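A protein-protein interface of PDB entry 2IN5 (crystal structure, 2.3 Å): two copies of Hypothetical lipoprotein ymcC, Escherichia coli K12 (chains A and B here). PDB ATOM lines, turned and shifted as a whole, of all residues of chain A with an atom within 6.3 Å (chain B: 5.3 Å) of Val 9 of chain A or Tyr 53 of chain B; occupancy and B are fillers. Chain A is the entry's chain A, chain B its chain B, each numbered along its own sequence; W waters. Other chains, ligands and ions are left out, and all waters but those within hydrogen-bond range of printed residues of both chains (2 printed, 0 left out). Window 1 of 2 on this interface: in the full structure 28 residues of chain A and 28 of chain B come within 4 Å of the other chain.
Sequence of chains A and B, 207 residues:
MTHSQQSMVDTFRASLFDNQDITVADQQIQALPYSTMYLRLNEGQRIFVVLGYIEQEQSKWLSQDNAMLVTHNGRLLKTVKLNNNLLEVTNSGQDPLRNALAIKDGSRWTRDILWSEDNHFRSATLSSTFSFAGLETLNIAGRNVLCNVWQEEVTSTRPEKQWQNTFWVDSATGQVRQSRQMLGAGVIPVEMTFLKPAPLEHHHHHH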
ATOM      1  N   SER A   7      26.745  -9.245  29.046  1.00  0.00           N
ATOM      2  CA  SER A   7      26.342 -10.396  28.232  1.00  0.00           C
ATOM      3  C   SER A   7      27.555 -11.027  27.569  1.00  0.00           C
ATOM      4  O   SER A   7      28.598 -10.384  27.427  1.00  0.00           O
ATOM      5  CB  SER A   7      25.342  -9.989  27.140  1.00  0.00           C
ATOM      6  OG  SER A   7      25.965  -9.243  26.106  1.00  0.00           O
ATOM      7  N   MET A   8      27.407 -12.285  27.161  1.00  0.00           N
ATOM      8  CA  MET A   8      28.481 -13.004  26.493  1.00  0.00           C
ATOM      9  C   MET A   8      28.793 -12.381  25.153  1.00  0.00           C
ATOM     10  O   MET A   8      29.938 -12.348  24.720  1.00  0.00           O
ATOM     11  CB  MET A   8      28.106 -14.467  26.257  1.00  0.00           C
ATOM     12  CG  MET A   8      28.017 -15.336  27.489  1.00  0.00           C
ATOM     13  SD  MET A   8      28.140 -17.167  26.914  1.00  0.00           S
ATOM     14  CE  MET A   8      28.077 -18.071  28.599  1.00  0.00           C
ATOM     15  N   VAL A   9      27.770 -11.904  24.470  1.00  0.00           N
ATOM     16  CA  VAL A   9      28.017 -11.306  23.177  1.00  0.00           C
ATOM     17  C   VAL A   9      28.902 -10.079  23.315  1.00  0.00           C
ATOM     18  O   VAL A   9      29.867  -9.936  22.584  1.00  0.00           O
ATOM     19  CB  VAL A   9      26.697 -10.952  22.469  1.00  0.00           C
ATOM     20  CG1 VAL A   9      26.962 -10.045  21.272  1.00  0.00           C
ATOM     21  CG2 VAL A   9      26.027 -12.237  21.995  1.00  0.00           C
ATOM     22  N   ASP A  10      28.593  -9.204  24.262  1.00  0.00           N
ATOM     23  CA  ASP A  10      29.403  -8.009  24.446  1.00  0.00           C
ATOM     24  C   ASP A  10      30.821  -8.333  24.869  1.00  0.00           C
ATOM     25  O   ASP A  10      31.769  -7.760  24.353  1.00  0.00           O
ATOM     26  CB  ASP A  10      28.758  -7.090  25.471  1.00  0.00           C
ATOM     27  CG  ASP A  10      27.478  -6.486  24.964  1.00  0.00           C
ATOM     28  OD1 ASP A  10      27.507  -5.904  23.856  1.00  0.00           O
ATOM     29  OD2 ASP A  10      26.445  -6.584  25.668  1.00  0.00           O
ATOM     30  N   THR A  11      30.957  -9.254  25.810  1.00  0.00           N
ATOM     31  CA  THR A  11      32.261  -9.649  26.310  1.00  0.00           C
ATOM     32  C   THR A  11      33.176 -10.252  25.238  1.00  0.00           C
ATOM     33  O   THR A  11      34.329  -9.828  25.084  1.00  0.00           O
ATOM     34  CB  THR A  11      32.109 -10.648  27.449  1.00  0.00           C
ATOM     35  OG1 THR A  11      31.571  -9.970  28.585  1.00  0.00           O
ATOM     36  CG2 THR A  11      33.446 -11.262  27.810  1.00  0.00           C
ATOM     37  N   PHE A  12      32.670 -11.238  24.503  1.00  0.00           N
ATOM     38  CA  PHE A  12      33.453 -11.887  23.465  1.00  0.00           C
ATOM     39  C   PHE A  12      33.599 -11.030  22.221  1.00  0.00           C
ATOM     40  O   PHE A  12      34.552 -11.187  21.467  1.00  0.00           O
ATOM     41  CB  PHE A  12      32.842 -13.252  23.140  1.00  0.00           C
ATOM     42  CG  PHE A  12      33.100 -14.281  24.203  1.00  0.00           C
ATOM     43  CD1 PHE A  12      34.217 -15.107  24.130  1.00  0.00           C
ATOM     44  CD2 PHE A  12      32.274 -14.371  25.316  1.00  0.00           C
ATOM     45  CE1 PHE A  12      34.515 -16.006  25.155  1.00  0.00           C
ATOM     46  CE2 PHE A  12      32.559 -15.269  26.354  1.00  0.00           C
ATOM     47  CZ  PHE A  12      33.687 -16.087  26.271  1.00  0.00           C
ATOM     48  N   ARG A  13      32.666 -10.106  22.021  1.00  0.00           N
ATOM     49  CA  ARG A  13      32.734  -9.214  20.877  1.00  0.00           C
ATOM     50  C   ARG A  13      33.845  -8.196  21.137  1.00  0.00           C
ATOM     51  O   ARG A  13      34.630  -7.884  20.247  1.00  0.00           O
ATOM     52  CB  ARG A  13      31.395  -8.495  20.683  1.00  0.00           C
ATOM     53  CG  ARG A  13      31.339  -7.515  19.514  1.00  0.00           C
ATOM     54  CD  ARG A  13      29.899  -7.071  19.265  1.00  0.00           C
ATOM     55  NE  ARG A  13      29.328  -6.448  20.457  1.00  0.00           N
ATOM     56  CZ  ARG A  13      29.379  -5.148  20.717  1.00  0.00           C
ATOM     57  NH1 ARG A  13      29.965  -4.322  19.861  1.00  0.00           N
ATOM     58  NH2 ARG A  13      28.866  -4.677  21.845  1.00  0.00           N
ATOM     59  N   ALA A  14      33.916  -7.686  22.364  1.00  0.00           N
ATOM     60  CA  ALA A  14      34.946  -6.708  22.712  1.00  0.00           C
ATOM     61  C   ALA A  14      36.319  -7.354  22.588  1.00  0.00           C
ATOM     62  O   ALA A  14      37.236  -6.789  21.986  1.00  0.00           O
ATOM     63  CB  ALA A  14      34.739  -6.197  24.127  1.00  0.00           C
ATOM     64  N   GLY A  52      26.099 -11.801  15.588  1.00  0.00           N
ATOM     65  CA  GLY A  52      25.837 -12.041  16.992  1.00  0.00           C
ATOM     66  C   GLY A  52      24.793 -13.113  17.237  1.00  0.00           C
ATOM     67  O   GLY A  52      25.017 -14.014  18.037  1.00  0.00           O
ATOM     68  N   TYR A  53      23.658 -13.033  16.551  1.00  0.00           N
ATOM     69  CA  TYR A  53      22.606 -14.016  16.771  1.00  0.00           C
ATOM     70  C   TYR A  53      21.525 -13.987  15.714  1.00  0.00           C
ATOM     71  O   TYR A  53      21.443 -13.051  14.918  1.00  0.00           O
ATOM     72  CB  TYR A  53      21.990 -13.797  18.150  1.00  0.00           C
ATOM     73  CG  TYR A  53      21.718 -12.339  18.462  1.00  0.00           C
ATOM     74  CD1 TYR A  53      20.549 -11.715  18.027  1.00  0.00           C
ATOM     75  CD2 TYR A  53      22.641 -11.579  19.176  1.00  0.00           C
ATOM     76  CE1 TYR A  53      20.308 -10.369  18.299  1.00  0.00           C
ATOM     77  CE2 TYR A  53      22.410 -10.234  19.449  1.00  0.00           C
ATOM     78  CZ  TYR A  53      21.246  -9.637  19.011  1.00  0.00           C
ATOM     79  OH  TYR A  53      21.018  -8.313  19.306  1.00  0.00           O
ATOM     80  N   ILE A  54      20.697 -15.023  15.697  1.00  0.00           N
ATOM     81  CA  ILE A  54      19.624 -15.092  14.707  1.00  0.00           C
ATOM     82  C   ILE A  54      18.275 -15.268  15.382  1.00  0.00           C
ATOM     83  O   ILE A  54      18.119 -16.112  16.257  1.00  0.00           O
ATOM     84  CB  ILE A  54      19.849 -16.260  13.719  1.00  0.00           C
ATOM     85  CG1 ILE A  54      21.258 -16.166  13.115  1.00  0.00           C
ATOM     86  CG2 ILE A  54      18.801 -16.224  12.621  1.00  0.00           C
ATOM     87  CD1 ILE A  54      21.631 -17.349  12.238  1.00  0.00           C
ATOM     88  N   GLU A  55      17.308 -14.455  14.966  1.00  0.00           N
ATOM     89  CA  GLU A  55      15.952 -14.493  15.505  1.00  0.00           C
ATOM     90  C   GLU A  55      14.931 -14.465  14.368  1.00  0.00           C
ATOM     91  O   GLU A  55      14.955 -13.572  13.524  1.00  0.00           O
ATOM     92  CB  GLU A  55      15.726 -13.300  16.441  1.00  0.00           C
ATOM     93  CG  GLU A  55      16.413 -13.449  17.797  1.00  0.00           C
ATOM     94  CD  GLU A  55      16.331 -12.195  18.661  1.00  0.00           C
ATOM     95  OE1 GLU A  55      16.654 -12.284  19.871  1.00  0.00           O
ATOM     96  OE2 GLU A  55      15.957 -11.123  18.130  1.00  0.00           O
ATOM     97  N   LEU A  62      26.694  -7.428  14.447  1.00  0.00           N
ATOM     98  CA  LEU A  62      27.151  -6.377  15.346  1.00  0.00           C
ATOM     99  C   LEU A  62      28.531  -5.835  15.012  1.00  0.00           C
ATOM    100  O   LEU A  62      29.455  -6.600  14.763  1.00  0.00           O
ATOM    101  CB  LEU A  62      27.174  -6.921  16.767  1.00  0.00           C
ATOM    102  CG  LEU A  62      25.816  -7.370  17.295  1.00  0.00           C
ATOM    103  CD1 LEU A  62      25.997  -8.187  18.554  1.00  0.00           C
ATOM    104  CD2 LEU A  62      24.950  -6.149  17.543  1.00  0.00           C
ATOM    105  N   MET B   8      27.551 -16.157  16.974  1.00  0.00           N
ATOM    106  CA  MET B   8      28.290 -16.247  18.223  1.00  0.00           C
ATOM    107  C   MET B   8      27.515 -17.038  19.276  1.00  0.00           C
ATOM    108  O   MET B   8      28.111 -17.729  20.099  1.00  0.00           O
ATOM    109  CB  MET B   8      28.587 -14.849  18.768  1.00  0.00           C
ATOM    110  CG  MET B   8      29.573 -14.006  17.956  1.00  0.00           C
ATOM    111  SD  MET B   8      30.093 -12.398  18.989  1.00  0.00           S
ATOM    112  CE  MET B   8      31.558 -13.209  19.971  1.00  0.00           C
ATOM    113  N   VAL B   9      26.187 -16.935  19.276  1.00  0.00           N
ATOM    114  CA  VAL B   9      25.408 -17.683  20.263  1.00  0.00           C
ATOM    115  C   VAL B   9      25.504 -19.176  19.984  1.00  0.00           C
ATOM    116  O   VAL B   9      25.579 -19.980  20.907  1.00  0.00           O
ATOM    117  CB  VAL B   9      23.924 -17.242  20.286  1.00  0.00           C
ATOM    118  CG1 VAL B   9      23.129 -18.143  21.231  1.00  0.00           C
ATOM    119  CG2 VAL B   9      23.834 -15.799  20.758  1.00  0.00           C
ATOM    120  N   PHE B  12      28.766 -20.126  21.421  1.00  0.00           N
ATOM    121  CA  PHE B  12      28.779 -20.172  22.880  1.00  0.00           C
ATOM    122  C   PHE B  12      28.067 -21.442  23.318  1.00  0.00           C
ATOM    123  O   PHE B  12      28.536 -22.134  24.213  1.00  0.00           O
ATOM    124  CB  PHE B  12      28.074 -18.960  23.495  1.00  0.00           C
ATOM    125  CG  PHE B  12      28.699 -17.646  23.140  1.00  0.00           C
ATOM    126  CD1 PHE B  12      30.067 -17.555  22.877  1.00  0.00           C
ATOM    127  CD2 PHE B  12      27.916 -16.494  23.052  1.00  0.00           C
ATOM    128  CE1 PHE B  12      30.642 -16.335  22.519  1.00  0.00           C
ATOM    129  CE2 PHE B  12      28.479 -15.269  22.696  1.00  0.00           C
ATOM    130  CZ  PHE B  12      29.843 -15.190  22.428  1.00  0.00           C
ATOM    131  N   LEU B  51      23.995 -15.287  30.354  1.00  0.00           N
ATOM    132  CA  LEU B  51      23.419 -14.193  29.593  1.00  0.00           C
ATOM    133  C   LEU B  51      24.082 -14.113  28.228  1.00  0.00           C
ATOM    134  O   LEU B  51      25.274 -13.836  28.125  1.00  0.00           O
ATOM    135  CB  LEU B  51      23.612 -12.876  30.355  1.00  0.00           C
ATOM    136  CG  LEU B  51      23.153 -11.588  29.665  1.00  0.00           C
ATOM    137  CD1 LEU B  51      21.651 -11.656  29.390  1.00  0.00           C
ATOM    138  CD2 LEU B  51      23.482 -10.399  30.539  1.00  0.00           C
ATOM    139  N   GLY B  52      23.299 -14.348  27.178  1.00  0.00           N
ATOM    140  CA  GLY B  52      23.836 -14.303  25.834  1.00  0.00           C
ATOM    141  C   GLY B  52      23.920 -12.907  25.251  1.00  0.00           C
ATOM    142  O   GLY B  52      24.954 -12.506  24.697  1.00  0.00           O
ATOM    143  N   TYR B  53      22.846 -12.148  25.369  1.00  0.00           N
ATOM    144  CA  TYR B  53      22.871 -10.815  24.818  1.00  0.00           C
ATOM    145  C   TYR B  53      21.690 -10.010  25.310  1.00  0.00           C
ATOM    146  O   TYR B  53      20.823 -10.535  26.010  1.00  0.00           O
ATOM    147  CB  TYR B  53      22.875 -10.891  23.295  1.00  0.00           C
ATOM    148  CG  TYR B  53      21.705 -11.639  22.678  1.00  0.00           C
ATOM    149  CD1 TYR B  53      20.541 -10.967  22.317  1.00  0.00           C
ATOM    150  CD2 TYR B  53      21.787 -13.008  22.406  1.00  0.00           C
ATOM    151  CE1 TYR B  53      19.487 -11.628  21.687  1.00  0.00           C
ATOM    152  CE2 TYR B  53      20.738 -13.688  21.780  1.00  0.00           C
ATOM    153  CZ  TYR B  53      19.592 -12.986  21.418  1.00  0.00           C
ATOM    154  OH  TYR B  53      18.565 -13.630  20.761  1.00  0.00           O
ATOM    155  N   ILE B  54      21.671  -8.732  24.958  1.00  0.00           N
ATOM    156  CA  ILE B  54      20.604  -7.855  25.380  1.00  0.00           C
ATOM    157  C   ILE B  54      20.167  -7.043  24.191  1.00  0.00           C
ATOM    158  O   ILE B  54      20.995  -6.616  23.392  1.00  0.00           O
ATOM    159  CB  ILE B  54      21.073  -6.908  26.496  1.00  0.00           C
ATOM    160  CG1 ILE B  54      21.606  -7.724  27.671  1.00  0.00           C
ATOM    161  CG2 ILE B  54      19.914  -6.027  26.955  1.00  0.00           C
ATOM    162  CD1 ILE B  54      22.253  -6.887  28.745  1.00  0.00           C
ATOM    163  N   GLU B  55      18.860  -6.852  24.067  1.00  0.00           N
ATOM    164  CA  GLU B  55      18.291  -6.088  22.967  1.00  0.00           C
ATOM    165  C   GLU B  55      16.988  -5.458  23.421  1.00  0.00           C
ATOM    166  O   GLU B  55      16.135  -6.131  24.005  1.00  0.00           O
ATOM    167  CB  GLU B  55      18.018  -6.989  21.759  1.00  0.00           C
ATOM    168  CG  GLU B  55      17.506  -6.219  20.544  1.00  0.00           C
ATOM    169  CD  GLU B  55      17.189  -7.105  19.338  1.00  0.00           C
ATOM    170  OE1 GLU B  55      16.892  -6.541  18.261  1.00  0.00           O
ATOM    171  OE2 GLU B  55      17.227  -8.350  19.464  1.00  0.00           O
ATOM    172  N   GLN B  58      15.842  -5.957  26.840  1.00  0.00           N
ATOM    173  CA  GLN B  58      15.484  -7.316  27.229  1.00  0.00           C
ATOM    174  C   GLN B  58      16.717  -8.205  27.334  1.00  0.00           C
ATOM    175  O   GLN B  58      17.570  -8.204  26.452  1.00  0.00           O
ATOM    176  CB  GLN B  58      14.513  -7.924  26.221  1.00  0.00           C
ATOM    177  CG  GLN B  58      13.202  -7.176  26.079  1.00  0.00           C
ATOM    178  CD  GLN B  58      12.230  -7.890  25.152  1.00  0.00           C
ATOM    179  OE1 GLN B  58      12.534  -8.142  23.977  1.00  0.00           O
ATOM    180  NE2 GLN B  58      11.049  -8.216  25.675  1.00  0.00           N
ATOM    181  N   SER B  59      16.805  -8.968  28.415  1.00  0.00           N
ATOM    182  CA  SER B  59      17.932  -9.861  28.610  1.00  0.00           C
ATOM    183  C   SER B  59      17.576 -11.262  28.136  1.00  0.00           C
ATOM    184  O   SER B  59      16.601 -11.855  28.600  1.00  0.00           O
ATOM    185  CB  SER B  59      18.337  -9.881  30.090  1.00  0.00           C
ATOM    186  OG  SER B  59      18.651  -8.576  30.529  1.00  0.00           O
ATOM    187  N   LYS B  60      18.366 -11.778  27.197  1.00  0.00           N
ATOM    188  CA  LYS B  60      18.154 -13.112  26.646  1.00  0.00           C
ATOM    189  C   LYS B  60      19.178 -14.088  27.203  1.00  0.00           C
ATOM    190  O   LYS B  60      20.348 -14.045  26.845  1.00  0.00           O
ATOM    191  CB  LYS B  60      18.269 -13.087  25.118  1.00  0.00           C
ATOM    192  CG  LYS B  60      17.007 -12.663  24.370  1.00  0.00           C
ATOM    193  CD  LYS B  60      16.740 -11.180  24.475  1.00  0.00           C
ATOM    194  CE  LYS B  60      15.585 -10.764  23.575  1.00  0.00           C
ATOM    195  NZ  LYS B  60      15.861 -11.028  22.152  1.00  0.00           N
ATOM    196  N   LEU B  62      20.796 -17.930  27.918  1.00  0.00           N
ATOM    197  CA  LEU B  62      20.987 -19.168  27.175  1.00  0.00           C
ATOM    198  C   LEU B  62      21.015 -20.338  28.134  1.00  0.00           C
ATOM    199  O   LEU B  62      21.715 -20.303  29.143  1.00  0.00           O
ATOM    200  CB  LEU B  62      22.298 -19.127  26.391  1.00  0.00           C
ATOM    201  CG  LEU B  62      22.565 -17.854  25.590  1.00  0.00           C
ATOM    202  CD1 LEU B  62      23.901 -18.000  24.888  1.00  0.00           C
ATOM    203  CD2 LEU B  62      21.452 -17.587  24.602  1.00  0.00           C
ATOM    204  N   MET B  68      15.900 -20.839  25.863  1.00  0.00           N
ATOM    205  CA  MET B  68      16.153 -19.428  26.078  1.00  0.00           C
ATOM    206  C   MET B  68      15.125 -18.819  27.019  1.00  0.00           C
ATOM    207  O   MET B  68      13.971 -19.248  27.066  1.00  0.00           O
ATOM    208  CB  MET B  68      16.154 -18.684  24.737  1.00  0.00           C
ATOM    209  CG  MET B  68      16.522 -17.211  24.854  1.00  0.00           C
ATOM    210  SD  MET B  68      16.888 -16.316  23.163  1.00  0.00           S
ATOM    211  CE  MET B  68      15.237 -15.337  22.936  1.00  0.00           C
HETATM  212  O   HOH W   1      24.423  -7.940  24.470  1.00  0.00           O
HETATM  213  O   HOH W   2      14.486  -8.296  19.532  1.00  0.00           O
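Printed residues of chain B within 4 Å of Met 8 of chain A: Phe 12 (3.7 Å), Leu 51 (2.8 Å) and Gly 52 (3.5 Å). Of the printed residues of chain B, Val 9 of chain A touches Phe 12, Gly 52 and Tyr 53. Leu 62 of chain A touches none of the printed residues of chain B. Printed residues of chain A within 4 Å of Phe 12 of chain B: Met 8 (3.7 Å), Val 9 (3.9 Å) and Phe 12 (3.6 Å). Of chain A, only Ser 7, Val 9, Tyr 53 and Glu 55 come within 4 Å of Tyr 53 of chain B. Ile 54 of chain B touches none of the printed residues of chain A. The nearest printed residue of chain B that does not touch Val 9 of chain A is Val 9 of chain B (4.4 Å). The nearest printed residue of chain A that does not touch Glu 55 of chain B is Asp 10 of chain A (7.8 Å).
Met 8 of chain A touches Phe 12 of chain B, and with the chains exchanged Phe 12 of chain A touches Met 8 of chain B. Val 9 of chain A touches Gly 52 of chain B, and with the chains exchanged Gly 52 of chain A touches Val 9 of chain B. Phe 12 of chain B touches its own counterpart, Phe 12 of chain A. Glu 55 of chain A touches its own counterpart, Glu 55 of chain B. Of the 20 pairs that touch across the chains among the printed residues, 13 have their exchanged pair printed and touching as well.
Water W1 lies within hydrogen-bond range of OG of Ser 7 of chain A (2.6 Å), OD2 of Asp 10 of chain A (2.7 Å) and N of Ile 54 of chain B (2.9 Å). Water W2 lies within hydrogen-bond range of OE2 of Glu 55 of chain B (2.7 Å) and OE2 of Glu 55 of chain A (3.5 Å).
N of Gly 52 of chain B is in hydrogen-bond range of O of Lys 60 of chain B (3.0 Å). The side-chain hydroxyl of Ser 7 of chain A sits at hydrogen-bond distance from the side-chain carboxylate of Asp 10 of chain A (2.7 Å). The backbone carbonyl oxygen of Tyr 53 of chain B sits at hydrogen-bond distance from the backbone NH of Lys 60 of chain B, at 3.0 Å. NH2 of Arg 13 of chain A is in salt-bridge range of OD1 of Asp 10 of chain A, at 2.7 Å. The side-chain hydroxyl (OG1) of Thr 11 of chain A is in hydrogen-bond range of the backbone carbonyl oxygen (O) of Ser 7 of chain A.
The backbone carbonyl oxygen of Gly 52 of chain B is in hydrogen-bond range of the backbone NH of Met 8 of chain A (3.5 Å). The backbone NH of Val 9 of chain B lies within hydrogen-bond range of the backbone carbonyl oxygen of Gly 52 of chain A, 3.4 Å away. The backbone NH (N) of Val 9 of chain A is in hydrogen-bond range of the backbone carbonyl oxygen (O) of Gly 52 of chain B (2.9 Å). OE2 of Glu 55 of chain A lies close to OE2 of Glu 55 of chain B, at 3.3 Å. O of Gly 52 of chain A is in hydrogen-bond range of N of Met 8 of chain B, at 3.5 Å. The backbone carbonyl oxygen (O) of Leu 51 of chain B is in hydrogen-bond range of the backbone NH (N) of Met 8 of chain A (2.8 Å). The side-chain carboxylate (OE1) of Glu 55 of chain A sits at hydrogen-bond distance from the side-chain hydroxyl (OH) of Tyr 53 of chain B (2.5 Å). The side-chain amino group of Lys 60 of chain B lies within salt-bridge range of the side-chain carboxylate of Glu 55 of chain A.
Of the 13 printed residues of chain B, 8 touch a printed residue of chain A. Along chain B the printed residues that touch a printed residue of chain A span positions 8 to 60. Printed residues of chain A that touch a printed residue of chain B: Ser 7, Met 8, Val 9, Phe 12, Arg 13, Gly 52, Tyr 53 and Glu 55. Among the printed residues, Asp or Glu carboxylates within 4 Å of a Lys or Arg side-chain nitrogen of the other chain: Glu 55 of chain A with Lys 60 of chain B (2.7 Å).
Ser 7 of chain A touches Gly 52 of chain B. Met 8 of chain A touches Phe 12 of chain B (O to CZ, 3.7 Å). Val 9 of chain A touches Phe 12 of chain B (N to CE2, 3.9 Å). Tyr 53 of chain B touches Val 9 of chain A (CB to CG2, 3.7 Å). Phe 12 of chain A touches Met 8 of chain B (CB to CE, 3.4 Å). Phe 12 of chain B touches Phe 12 of chain A (CE1 to CG, 3.6 Å). N of Arg 13 of chain A touches CE of Met 8 of chain B, at 3.9 Å. CG2 of Val 9 of chain B touches CB of Tyr 53 of chain A (3.8 Å). CE2 of Tyr 53 of chain A touches CD1 of Tyr 53 of chain B (3.5 Å). OH of Tyr 53 of chain A touches OE2 of Glu 55 of chain B, 3.8 Å away.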
